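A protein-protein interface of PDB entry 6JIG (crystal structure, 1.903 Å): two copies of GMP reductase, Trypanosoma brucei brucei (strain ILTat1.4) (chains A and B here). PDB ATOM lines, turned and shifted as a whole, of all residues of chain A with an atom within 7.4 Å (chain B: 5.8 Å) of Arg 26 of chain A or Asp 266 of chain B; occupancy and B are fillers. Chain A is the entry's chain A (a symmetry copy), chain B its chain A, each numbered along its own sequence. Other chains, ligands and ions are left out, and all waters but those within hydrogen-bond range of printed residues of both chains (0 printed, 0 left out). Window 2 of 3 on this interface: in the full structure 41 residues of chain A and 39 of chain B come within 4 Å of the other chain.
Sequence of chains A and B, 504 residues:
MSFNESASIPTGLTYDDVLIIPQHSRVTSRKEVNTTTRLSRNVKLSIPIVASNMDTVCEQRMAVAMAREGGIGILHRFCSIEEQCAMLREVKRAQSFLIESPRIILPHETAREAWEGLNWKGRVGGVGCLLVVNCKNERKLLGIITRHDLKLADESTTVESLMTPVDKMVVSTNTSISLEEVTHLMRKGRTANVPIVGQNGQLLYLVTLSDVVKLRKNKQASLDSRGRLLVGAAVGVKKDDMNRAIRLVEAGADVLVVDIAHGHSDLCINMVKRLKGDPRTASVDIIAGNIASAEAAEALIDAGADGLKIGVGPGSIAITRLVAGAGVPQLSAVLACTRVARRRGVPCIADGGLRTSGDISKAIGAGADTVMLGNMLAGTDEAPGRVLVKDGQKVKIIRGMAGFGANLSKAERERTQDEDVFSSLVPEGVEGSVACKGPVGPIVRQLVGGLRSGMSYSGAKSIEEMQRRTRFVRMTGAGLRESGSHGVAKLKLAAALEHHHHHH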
ATOM      1  N   GLN A  23      19.791 -23.633   3.872  1.00  0.00           N
ATOM      2  CA  GLN A  23      18.748 -24.470   4.446  1.00  0.00           C
ATOM      3  C   GLN A  23      17.555 -23.592   4.792  1.00  0.00           C
ATOM      4  O   GLN A  23      17.631 -22.362   4.767  1.00  0.00           O
ATOM      5  CB  GLN A  23      19.223 -25.189   5.721  1.00  0.00           C
ATOM      6  CG  GLN A  23      20.515 -25.972   5.581  1.00  0.00           C
ATOM      7  CD  GLN A  23      20.353 -27.173   4.662  1.00  0.00           C
ATOM      8  OE1 GLN A  23      19.436 -27.981   4.832  1.00  0.00           O
ATOM      9  NE2 GLN A  23      21.253 -27.301   3.687  1.00  0.00           N
ATOM     10  N   HIS A  24      16.442 -24.242   5.100  1.00  0.00           N
ATOM     11  CA  HIS A  24      15.275 -23.509   5.572  1.00  0.00           C
ATOM     12  C   HIS A  24      15.596 -22.770   6.865  1.00  0.00           C
ATOM     13  O   HIS A  24      16.035 -23.375   7.847  1.00  0.00           O
ATOM     14  CB  HIS A  24      14.115 -24.472   5.791  1.00  0.00           C
ATOM     15  CG  HIS A  24      12.902 -23.821   6.376  1.00  0.00           C
ATOM     16  ND1 HIS A  24      12.364 -22.659   5.867  1.00  0.00           N
ATOM     17  CD2 HIS A  24      12.135 -24.160   7.438  1.00  0.00           C
ATOM     18  CE1 HIS A  24      11.310 -22.313   6.584  1.00  0.00           C
ATOM     19  NE2 HIS A  24      11.148 -23.208   7.542  1.00  0.00           N
ATOM     20  N   SER A  25      15.366 -21.459   6.876  1.00  0.00           N
ATOM     21  CA  SER A  25      15.690 -20.632   8.028  1.00  0.00           C
ATOM     22  C   SER A  25      14.401 -20.075   8.621  1.00  0.00           C
ATOM     23  O   SER A  25      13.650 -19.369   7.938  1.00  0.00           O
ATOM     24  CB  SER A  25      16.639 -19.498   7.630  1.00  0.00           C
ATOM     25  OG  SER A  25      16.758 -18.530   8.652  1.00  0.00           O
ATOM     26  N   ARG A  26      14.146 -20.401   9.883  1.00  0.00           N
ATOM     27  CA  ARG A  26      13.090 -19.741  10.634  1.00  0.00           C
ATOM     28  C   ARG A  26      13.594 -18.481  11.319  1.00  0.00           C
ATOM     29  O   ARG A  26      12.823 -17.809  12.014  1.00  0.00           O
ATOM     30  CB  ARG A  26      12.495 -20.708  11.661  1.00  0.00           C
ATOM     31  CG  ARG A  26      13.398 -20.940  12.869  1.00  0.00           C
ATOM     32  CD  ARG A  26      13.163 -22.305  13.511  1.00  0.00           C
ATOM     33  NE  ARG A  26      13.885 -22.450  14.776  1.00  0.00           N
ATOM     34  CZ  ARG A  26      15.178 -22.751  14.873  1.00  0.00           C
ATOM     35  NH1 ARG A  26      15.897 -22.939  13.774  1.00  0.00           N
ATOM     36  NH2 ARG A  26      15.756 -22.867  16.064  1.00  0.00           N
ATOM     37  N   VAL A  27      14.874 -18.156  11.135  1.00  0.00           N
ATOM     38  CA  VAL A  27      15.475 -16.999  11.789  1.00  0.00           C
ATOM     39  C   VAL A  27      14.822 -15.737  11.256  1.00  0.00           C
ATOM     40  O   VAL A  27      14.898 -15.440  10.058  1.00  0.00           O
ATOM     41  CB  VAL A  27      16.991 -16.970  11.555  1.00  0.00           C
ATOM     42  CG1 VAL A  27      17.605 -15.762  12.251  1.00  0.00           C
ATOM     43  CG2 VAL A  27      17.659 -18.292  12.000  1.00  0.00           C
ATOM     44  N   THR A  28      14.178 -14.980  12.140  1.00  0.00           N
ATOM     45  CA  THR A  28      13.598 -13.709  11.730  1.00  0.00           C
ATOM     46  C   THR A  28      14.480 -12.522  12.084  1.00  0.00           C
ATOM     47  O   THR A  28      14.617 -11.601  11.275  1.00  0.00           O
ATOM     48  CB  THR A  28      12.206 -13.534  12.343  1.00  0.00           C
ATOM     49  OG1 THR A  28      12.290 -13.595  13.772  1.00  0.00           O
ATOM     50  CG2 THR A  28      11.282 -14.640  11.850  1.00  0.00           C
ATOM     51  N   SER A  29      15.109 -12.529  13.256  1.00  0.00           N
ATOM     52  CA  SER A  29      15.980 -11.441  13.679  1.00  0.00           C
ATOM     53  C   SER A  29      17.422 -11.922  13.778  1.00  0.00           C
ATOM     54  O   SER A  29      17.692 -13.031  14.259  1.00  0.00           O
ATOM     55  CB  SER A  29      15.527 -10.864  15.025  1.00  0.00           C
ATOM     56  N   GLU A  32      18.342 -13.254  17.198  1.00  0.00           N
ATOM     57  CA  GLU A  32      17.958 -14.569  17.705  1.00  0.00           C
ATOM     58  C   GLU A  32      19.072 -15.609  17.611  1.00  0.00           C
ATOM     59  O   GLU A  32      18.887 -16.727  18.104  1.00  0.00           O
ATOM     60  CB  GLU A  32      16.723 -15.101  16.961  1.00  0.00           C
ATOM     61  CG  GLU A  32      15.700 -14.048  16.576  1.00  0.00           C
ATOM     62  CD  GLU A  32      14.473 -14.634  15.874  1.00  0.00           C
ATOM     63  OE1 GLU A  32      14.605 -15.657  15.166  1.00  0.00           O
ATOM     64  OE2 GLU A  32      13.371 -14.066  16.031  1.00  0.00           O
ATOM     65  N   SER A 456      22.499 -18.347   9.978  1.00  0.00           N
ATOM     66  CA  SER A 456      21.181 -18.102   9.402  1.00  0.00           C
ATOM     67  C   SER A 456      20.988 -18.873   8.099  1.00  0.00           C
ATOM     68  O   SER A 456      19.878 -19.329   7.800  1.00  0.00           O
ATOM     69  CB  SER A 456      20.991 -16.609   9.172  1.00  0.00           C
ATOM     70  OG  SER A 456      19.708 -16.354   8.626  1.00  0.00           O
ATOM     71  N   SER A 458      22.211 -21.779   7.479  1.00  0.00           N
ATOM     72  CA  SER A 458      21.972 -23.157   7.889  1.00  0.00           C
ATOM     73  C   SER A 458      20.681 -23.312   8.679  1.00  0.00           C
ATOM     74  O   SER A 458      20.366 -24.431   9.102  1.00  0.00           O
ATOM     75  CB  SER A 458      23.150 -23.692   8.730  1.00  0.00           C
ATOM     76  OG  SER A 458      24.249 -24.084   7.892  1.00  0.00           O
ATOM     77  N   GLY A 459      19.950 -22.224   8.889  1.00  0.00           N
ATOM     78  CA  GLY A 459      18.747 -22.239   9.708  1.00  0.00           C
ATOM     79  C   GLY A 459      19.012 -22.500  11.173  1.00  0.00           C
ATOM     80  O   GLY A 459      18.147 -23.051  11.863  1.00  0.00           O
ATOM     81  N   ALA A 460      20.193 -22.128  11.668  1.00  0.00           N
ATOM     82  CA  ALA A 460      20.640 -22.478  13.012  1.00  0.00           C
ATOM     83  C   ALA A 460      20.552 -21.265  13.928  1.00  0.00           C
ATOM     84  O   ALA A 460      21.035 -20.182  13.578  1.00  0.00           O
ATOM     85  CB  ALA A 460      22.085 -22.998  12.984  1.00  0.00           C
ATOM     86  N   LYS A 461      19.958 -21.448  15.113  1.00  0.00           N
ATOM     87  CA  LYS A 461      19.925 -20.394  16.117  1.00  0.00           C
ATOM     88  C   LYS A 461      20.951 -20.599  17.233  1.00  0.00           C
ATOM     89  O   LYS A 461      21.013 -19.782  18.162  1.00  0.00           O
ATOM     90  CB  LYS A 461      18.514 -20.276  16.716  1.00  0.00           C
ATOM     91  N   SER A 462      21.751 -21.662  17.169  1.00  0.00           N
ATOM     92  CA  SER A 462      22.748 -21.952  18.188  1.00  0.00           C
ATOM     93  C   SER A 462      23.940 -22.626  17.522  1.00  0.00           C
ATOM     94  O   SER A 462      23.857 -23.083  16.376  1.00  0.00           O
ATOM     95  CB  SER A 462      22.189 -22.866  19.284  1.00  0.00           C
ATOM     96  OG  SER A 462      21.975 -24.175  18.766  1.00  0.00           O
ATOM     97  N   GLU A 465      23.100 -26.269  16.928  1.00  0.00           N
ATOM     98  CA  GLU A 465      22.260 -26.396  15.738  1.00  0.00           C
ATOM     99  C   GLU A 465      23.077 -26.202  14.464  1.00  0.00           C
ATOM    100  O   GLU A 465      22.832 -26.868  13.451  1.00  0.00           O
ATOM    101  CB  GLU A 465      21.119 -25.382  15.781  1.00  0.00           C
ATOM    102  CG  GLU A 465      19.970 -25.766  16.701  1.00  0.00           C
ATOM    103  CD  GLU A 465      18.852 -24.726  16.710  1.00  0.00           C
ATOM    104  OE1 GLU A 465      18.723 -23.964  15.720  1.00  0.00           O
ATOM    105  OE2 GLU A 465      18.093 -24.680  17.708  1.00  0.00           O
ATOM    106  N   ARG A 469      23.010 -29.072  11.709  1.00  0.00           N
ATOM    107  CA  ARG A 469      22.214 -28.802  10.517  1.00  0.00           C
ATOM    108  C   ARG A 469      23.044 -28.520   9.270  1.00  0.00           C
ATOM    109  O   ARG A 469      22.527 -28.657   8.158  1.00  0.00           O
ATOM    110  CB  ARG A 469      21.277 -27.620  10.770  1.00  0.00           C
ATOM    111  CG  ARG A 469      20.083 -28.012  11.619  1.00  0.00           C
ATOM    112  CD  ARG A 469      19.292 -26.836  12.163  1.00  0.00           C
ATOM    113  NE  ARG A 469      18.434 -27.335  13.245  1.00  0.00           N
ATOM    114  CZ  ARG A 469      17.620 -26.595  13.991  1.00  0.00           C
ATOM    115  NH1 ARG A 469      17.529 -25.290  13.787  1.00  0.00           N
ATOM    116  NH2 ARG A 469      16.897 -27.166  14.949  1.00  0.00           N
ATOM    117  N   HIS B 264      15.012 -18.921   1.024  1.00  0.00           N
ATOM    118  CA  HIS B 264      14.447 -20.089   1.712  1.00  0.00           C
ATOM    119  C   HIS B 264      14.283 -19.794   3.204  1.00  0.00           C
ATOM    120  O   HIS B 264      14.915 -20.396   4.072  1.00  0.00           O
ATOM    121  CB  HIS B 264      15.318 -21.319   1.494  1.00  0.00           C
ATOM    122  CG  HIS B 264      14.641 -22.609   1.843  1.00  0.00           C
ATOM    123  ND1 HIS B 264      15.298 -23.821   1.838  1.00  0.00           N
ATOM    124  CD2 HIS B 264      13.362 -22.875   2.201  1.00  0.00           C
ATOM    125  CE1 HIS B 264      14.456 -24.779   2.183  1.00  0.00           C
ATOM    126  NE2 HIS B 264      13.275 -24.229   2.415  1.00  0.00           N
ATOM    127  N   SER B 265      13.419 -18.836   3.496  1.00  0.00           N
ATOM    128  CA  SER B 265      13.230 -18.396   4.866  1.00  0.00           C
ATOM    129  C   SER B 265      11.762 -18.073   5.055  1.00  0.00           C
ATOM    130  O   SER B 265      11.054 -17.748   4.100  1.00  0.00           O
ATOM    131  CB  SER B 265      14.089 -17.173   5.178  1.00  0.00           C
ATOM    132  OG  SER B 265      13.703 -16.097   4.336  1.00  0.00           O
ATOM    133  N   ASP B 266      11.307 -18.160   6.306  1.00  0.00           N
ATOM    134  CA  ASP B 266       9.915 -17.825   6.589  1.00  0.00           C
ATOM    135  C   ASP B 266       9.603 -16.383   6.217  1.00  0.00           C
ATOM    136  O   ASP B 266       8.482 -16.085   5.790  1.00  0.00           O
ATOM    137  CB  ASP B 266       9.605 -18.102   8.059  1.00  0.00           C
ATOM    138  CG  ASP B 266       9.558 -19.589   8.358  1.00  0.00           C
ATOM    139  OD1 ASP B 266       9.365 -20.371   7.407  1.00  0.00           O
ATOM    140  OD2 ASP B 266       9.728 -19.979   9.526  1.00  0.00           O
ATOM    141  N   LEU B 267      10.583 -15.483   6.347  1.00  0.00           N
ATOM    142  CA  LEU B 267      10.375 -14.083   5.989  1.00  0.00           C
ATOM    143  C   LEU B 267       9.951 -13.953   4.535  1.00  0.00           C
ATOM    144  O   LEU B 267       9.029 -13.191   4.200  1.00  0.00           O
ATOM    145  CB  LEU B 267      11.656 -13.282   6.221  1.00  0.00           C
ATOM    146  CG  LEU B 267      12.062 -12.939   7.657  1.00  0.00           C
ATOM    147  CD1 LEU B 267      13.180 -11.920   7.626  1.00  0.00           C
ATOM    148  CD2 LEU B 267      10.883 -12.413   8.434  1.00  0.00           C
ATOM    149  N   CYS B 268      10.634 -14.683   3.652  1.00  0.00           N
ATOM    150  CA  CYS B 268      10.305 -14.607   2.236  1.00  0.00           C
ATOM    151  C   CYS B 268       9.013 -15.346   1.943  1.00  0.00           C
ATOM    152  O   CYS B 268       8.160 -14.850   1.202  1.00  0.00           O
ATOM    153  CB  CYS B 268      11.466 -15.195   1.405  1.00  0.00           C
ATOM    154  SG  CYS B 268      11.186 -15.124  -0.375  1.00  0.00           S
ATOM    155  N   ILE B 269       8.842 -16.534   2.522  1.00  0.00           N
ATOM    156  CA  ILE B 269       7.632 -17.314   2.279  1.00  0.00           C
ATOM    157  C   ILE B 269       6.392 -16.549   2.735  1.00  0.00           C
ATOM    158  O   ILE B 269       5.340 -16.577   2.079  1.00  0.00           O
ATOM    159  CB  ILE B 269       7.743 -18.675   2.987  1.00  0.00           C
ATOM    160  CG1 ILE B 269       8.712 -19.600   2.236  1.00  0.00           C
ATOM    161  CG2 ILE B 269       6.383 -19.329   3.158  1.00  0.00           C
ATOM    162  CD1 ILE B 269       9.265 -20.726   3.104  1.00  0.00           C
ATOM    163  N   ASN B 270       6.501 -15.856   3.866  1.00  0.00           N
ATOM    164  CA  ASN B 270       5.354 -15.133   4.405  1.00  0.00           C
ATOM    165  C   ASN B 270       5.072 -13.862   3.616  1.00  0.00           C
ATOM    166  O   ASN B 270       3.911 -13.450   3.502  1.00  0.00           O
ATOM    167  CB  ASN B 270       5.591 -14.828   5.884  1.00  0.00           C
ATOM    168  CG  ASN B 270       5.539 -16.075   6.738  1.00  0.00           C
ATOM    169  OD1 ASN B 270       4.927 -17.073   6.352  1.00  0.00           O
ATOM    170  ND2 ASN B 270       6.169 -16.028   7.906  1.00  0.00           N
ATOM    171  N   MET B 271       6.110 -13.234   3.055  1.00  0.00           N
ATOM    172  CA  MET B 271       5.878 -12.094   2.176  1.00  0.00           C
ATOM    173  C   MET B 271       5.156 -12.525   0.902  1.00  0.00           C
ATOM    174  O   MET B 271       4.240 -11.832   0.439  1.00  0.00           O
ATOM    175  CB  MET B 271       7.202 -11.404   1.844  1.00  0.00           C
ATOM    176  CG  MET B 271       7.038 -10.073   1.128  1.00  0.00           C
ATOM    177  SD  MET B 271       6.199  -8.875   2.204  1.00  0.00           S
ATOM    178  CE  MET B 271       6.046  -7.493   1.086  1.00  0.00           C
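A ring nitrogen (ND1) of His 264 of chain B is in hydrogen-bond range of the backbone NH of His 24 of chain A, 3.5 Å away. N of Ser 25 of chain A lies within hydrogen-bond range of O of His 264 of chain B, at 3.0 Å. OD1 of Asp 266 of chain B lies close to NE2 of His 24 of chain A, at 3.4 Å. The backbone NH (N) of Asp 266 of chain B is in hydrogen-bond range of the backbone carbonyl oxygen (O) of Ser 25 of chain A (3.1 Å). The backbone carbonyl oxygen (O) of Gln 23 of chain A lies close to the backbone carbonyl oxygen (O) of His 264 of chain B (3.4 Å).
Of the 8 printed residues of chain B, 4 touch a printed residue of chain A. Hydrophobic or aromatic side chains of chain A that line the printed part of chain B: His 24. Among the printed residues, no Asp or Glu carboxylate lies within 4 Å of a Lys or Arg side-chain nitrogen of the other chain.
Of chain B, only Asp 266 (3.5 Å) comes within 4 Å of Arg 26 of chain A. Asp 266 of chain B touches just these residues of chain A: His 24 (2.9 Å), Ser 25 (3.1 Å) and Arg 26 (3.5 Å). Printed residues of chain B within 4 Å of His 24 of chain A: His 264 (3.5 Å) and Asp 266 (2.9 Å). Of the printed residues of chain B, Ser 25 of chain A touches His 264, Ser 265 and Asp 266. Of the printed residues of chain B, Gln 23 of chain A touches His 264 (3.4 Å). Printed residues of chain A within 4 Å of Ser 265 of chain B: Ser 25. Of the printed residues of chain A, His 264 of chain B touches Gln 23 (3.4 Å), His 24 (3.5 Å) and Ser 25 (3.0 Å). Met 271 of chain B touches none of the printed residues of chain A. The nearest residue of chain B that does not touch Arg 26 of chain A is Ser 265 of chain B (5.5 Å). The nearest printed residue of chain B that does not touch Thr 28 of chain A is Asp 266 of chain B (5.4 Å).
No position is printed for both chains.
The side-chain hydroxyl (OG) of Ser 265 of chain B sits at hydrogen-bond distance from the backbone NH (N) of Cys 268 of chain B (3.4 Å). ND2 of Asn 270 of chain B sits close to O of Asp 266 of chain B, at 3.1 Å. OG of Ser 25 of chain A lies close to O of Ser 456 of chain A. NH1 of Arg 26 of chain A is in hydrogen-bond range of O of Gly 459 of chain A (3.0 Å). NH2 of Arg 26 of chain A lies within salt-bridge range of OE1 of Glu 465 of chain A (3.2 Å). The side-chain carboxylate (OE2) of Glu 32 of chain A lies within hydrogen-bond range of the side-chain hydroxyl (OG1) of Thr 28 of chain A (2.5 Å).
Among the printed residues, pairs that only touch across the chains: Ser 25 of chain A with Ser 265 of chain B (3.2 Å), Arg 26 of chain A with Asp 266 of chain B (3.5 Å) and Thr 28 of chain A with Leu 267 of chain B (3.9 Å).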
